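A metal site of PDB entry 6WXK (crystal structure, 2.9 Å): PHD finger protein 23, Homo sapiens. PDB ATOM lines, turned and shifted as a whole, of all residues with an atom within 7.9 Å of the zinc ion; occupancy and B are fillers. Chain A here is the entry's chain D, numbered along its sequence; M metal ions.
The backbone NH (N) of Leu 26 sits close to the side-chain sulfur (SG) of Cys 24 (3.7 Å).
The backbone carbonyl oxygen of Thr 29 sits at hydrogen-bond distance from the backbone NH of Cys 24 (2.7 Å).
SG of Cys 49 lies close to OH of Tyr 11, at 3.6 Å.
The side-chain sulfur (SG) of Cys 27 is disulfide-bonded to the side-chain sulfur (SG) of Cys 49, at 1.8 Å.
Three residues have an atom within 4 Å of the zinc ion: Cys 24, Cys 27 and Cys 49.
The zinc ion is bound by the side-chain sulfur of Cys 27 (2.0 Å), the side-chain sulfur of Cys 49 (2.4 Å) and the side-chain sulfur of Cys 24 (2.6 Å).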
ATOM      1  N   TYR A  11       2.628  20.668  -6.731  1.00  0.00           N
ATOM      2  CA  TYR A  11       1.902  20.649  -7.995  1.00  0.00           C
ATOM      3  C   TYR A  11       2.164  21.904  -8.822  1.00  0.00           C
ATOM      4  O   TYR A  11       1.877  21.898 -10.028  1.00  0.00           O
ATOM      5  CB  TYR A  11       0.412  20.505  -7.713  1.00  0.00           C
ATOM      6  CG  TYR A  11       0.057  19.186  -7.036  1.00  0.00           C
ATOM      7  CD1 TYR A  11       0.933  18.111  -7.065  1.00  0.00           C
ATOM      8  CD2 TYR A  11      -1.141  19.050  -6.341  1.00  0.00           C
ATOM      9  CE1 TYR A  11       0.625  16.910  -6.450  1.00  0.00           C
ATOM     10  CE2 TYR A  11      -1.462  17.854  -5.716  1.00  0.00           C
ATOM     11  CZ  TYR A  11      -0.582  16.788  -5.776  1.00  0.00           C
ATOM     12  OH  TYR A  11      -0.908  15.603  -5.144  1.00  0.00           O
ATOM     13  N   GLU A  23       3.397  18.266   4.383  1.00  0.00           N
ATOM     14  CA  GLU A  23       3.187  16.980   3.744  1.00  0.00           C
ATOM     15  C   GLU A  23       1.703  16.618   3.738  1.00  0.00           C
ATOM     16  O   GLU A  23       0.974  16.932   4.680  1.00  0.00           O
ATOM     17  CB  GLU A  23       3.991  15.863   4.423  1.00  0.00           C
ATOM     18  CG  GLU A  23       3.600  15.583   5.853  1.00  0.00           C
ATOM     19  CD  GLU A  23       4.396  14.423   6.439  1.00  0.00           C
ATOM     20  OE1 GLU A  23       5.194  13.813   5.700  1.00  0.00           O
ATOM     21  OE2 GLU A  23       4.232  14.143   7.644  1.00  0.00           O
ATOM     22  N   CYS A  24       1.284  15.970   2.664  1.00  0.00           N
ATOM     23  CA  CYS A  24      -0.030  15.354   2.591  1.00  0.00           C
ATOM     24  C   CYS A  24      -0.042  14.132   3.504  1.00  0.00           C
ATOM     25  O   CYS A  24       0.818  13.247   3.371  1.00  0.00           O
ATOM     26  CB  CYS A  24      -0.339  14.954   1.159  1.00  0.00           C
ATOM     27  SG  CYS A  24      -1.920  14.130   0.828  1.00  0.00           S
ATOM     28  N   SER A  25      -0.976  14.099   4.455  1.00  0.00           N
ATOM     29  CA  SER A  25      -0.993  12.984   5.410  1.00  0.00           C
ATOM     30  C   SER A  25      -1.274  11.652   4.718  1.00  0.00           C
ATOM     31  O   SER A  25      -0.915  10.609   5.264  1.00  0.00           O
ATOM     32  CB  SER A  25      -2.025  13.256   6.502  1.00  0.00           C
ATOM     33  OG  SER A  25      -2.013  12.216   7.464  1.00  0.00           O
ATOM     34  N   LEU A  26      -1.897  11.668   3.539  1.00  0.00           N
ATOM     35  CA  LEU A  26      -2.110  10.468   2.743  1.00  0.00           C
ATOM     36  C   LEU A  26      -1.038  10.278   1.668  1.00  0.00           C
ATOM     37  O   LEU A  26      -0.408   9.217   1.617  1.00  0.00           O
ATOM     38  CB  LEU A  26      -3.496  10.524   2.077  1.00  0.00           C
ATOM     39  N   CYS A  27      -0.813  11.294   0.831  1.00  0.00           N
ATOM     40  CA  CYS A  27       0.043  11.131  -0.350  1.00  0.00           C
ATOM     41  C   CYS A  27       1.517  11.046   0.007  1.00  0.00           C
ATOM     42  O   CYS A  27       2.293  10.416  -0.717  1.00  0.00           O
ATOM     43  CB  CYS A  27      -0.111  12.320  -1.277  1.00  0.00           C
ATOM     44  SG  CYS A  27      -1.748  12.755  -1.694  1.00  0.00           S
ATOM     45  N   GLY A  28       1.915  11.654   1.119  1.00  0.00           N
ATOM     46  CA  GLY A  28       3.323  11.842   1.408  1.00  0.00           C
ATOM     47  C   GLY A  28       3.917  13.040   0.691  1.00  0.00           C
ATOM     48  O   GLY A  28       5.057  13.420   0.988  1.00  0.00           O
ATOM     49  N   THR A  29       3.155  13.657  -0.226  1.00  0.00           N
ATOM     50  CA  THR A  29       3.648  14.720  -1.082  1.00  0.00           C
ATOM     51  C   THR A  29       3.832  16.016  -0.302  1.00  0.00           C
ATOM     52  O   THR A  29       3.071  16.321   0.610  1.00  0.00           O
ATOM     53  CB  THR A  29       2.650  14.945  -2.225  1.00  0.00           C
ATOM     54  OG1 THR A  29       2.470  13.718  -2.946  1.00  0.00           O
ATOM     55  CG2 THR A  29       3.138  16.020  -3.194  1.00  0.00           C
ATOM     56  N   PHE A  47      -3.083  17.541   6.785  1.00  0.00           N
ATOM     57  CA  PHE A  47      -3.207  18.165   5.479  1.00  0.00           C
ATOM     58  C   PHE A  47      -3.441  17.112   4.404  1.00  0.00           C
ATOM     59  O   PHE A  47      -2.952  15.981   4.508  1.00  0.00           O
ATOM     60  CB  PHE A  47      -1.951  18.957   5.156  1.00  0.00           C
ATOM     61  CG  PHE A  47      -1.945  19.535   3.777  1.00  0.00           C
ATOM     62  CD1 PHE A  47      -2.742  20.616   3.469  1.00  0.00           C
ATOM     63  CD2 PHE A  47      -1.127  18.999   2.803  1.00  0.00           C
ATOM     64  CE1 PHE A  47      -2.748  21.149   2.199  1.00  0.00           C
ATOM     65  CE2 PHE A  47      -1.124  19.536   1.532  1.00  0.00           C
ATOM     66  CZ  PHE A  47      -1.930  20.615   1.235  1.00  0.00           C
ATOM     67  N   TYR A  48      -4.190  17.483   3.346  1.00  0.00           N
ATOM     68  CA  TYR A  48      -4.501  16.519   2.296  1.00  0.00           C
ATOM     69  C   TYR A  48      -4.352  17.098   0.886  1.00  0.00           C
ATOM     70  O   TYR A  48      -4.912  18.157   0.582  1.00  0.00           O
ATOM     71  CB  TYR A  48      -5.927  15.993   2.492  1.00  0.00           C
ATOM     72  CG  TYR A  48      -6.094  15.348   3.842  1.00  0.00           C
ATOM     73  CD1 TYR A  48      -5.553  14.101   4.109  1.00  0.00           C
ATOM     74  CD2 TYR A  48      -6.766  16.005   4.867  1.00  0.00           C
ATOM     75  CE1 TYR A  48      -5.685  13.501   5.350  1.00  0.00           C
ATOM     76  CE2 TYR A  48      -6.916  15.420   6.115  1.00  0.00           C
ATOM     77  CZ  TYR A  48      -6.366  14.172   6.351  1.00  0.00           C
ATOM     78  OH  TYR A  48      -6.507  13.590   7.589  1.00  0.00           O
ATOM     79  N   CYS A  49      -3.571  16.397   0.062  1.00  0.00           N
ATOM     80  CA  CYS A  49      -3.266  16.788  -1.326  1.00  0.00           C
ATOM     81  C   CYS A  49      -4.263  16.181  -2.314  1.00  0.00           C
ATOM     82  O   CYS A  49      -3.960  15.224  -3.022  1.00  0.00           O
ATOM     83  CB  CYS A  49      -1.865  16.342  -1.708  1.00  0.00           C
ATOM     84  SG  CYS A  49      -1.787  14.520  -1.828  1.00  0.00           S
ATOM     85  N   GLN A  50      -5.467  16.740  -2.348  1.00  0.00           N
ATOM     86  CA  GLN A  50      -6.450  16.405  -3.394  1.00  0.00           C
ATOM     87  C   GLN A  50      -6.811  14.923  -3.451  1.00  0.00           C
ATOM     88  O   GLN A  50      -6.325  14.197  -4.310  1.00  0.00           O
ATOM     89  CB  GLN A  50      -5.927  16.838  -4.749  1.00  0.00           C
ATOM     90  CG  GLN A  50      -5.481  18.274  -4.756  1.00  0.00           C
ATOM     91  CD  GLN A  50      -6.545  19.190  -4.213  1.00  0.00           C
ATOM     92  OE1 GLN A  50      -6.449  19.686  -3.091  1.00  0.00           O
ATOM     93  NE2 GLN A  50      -7.577  19.432  -5.014  1.00  0.00           N
HETATM   94 ZN    ZN M   1      -3.523  13.185  -0.923  1.00  0.00          ZN
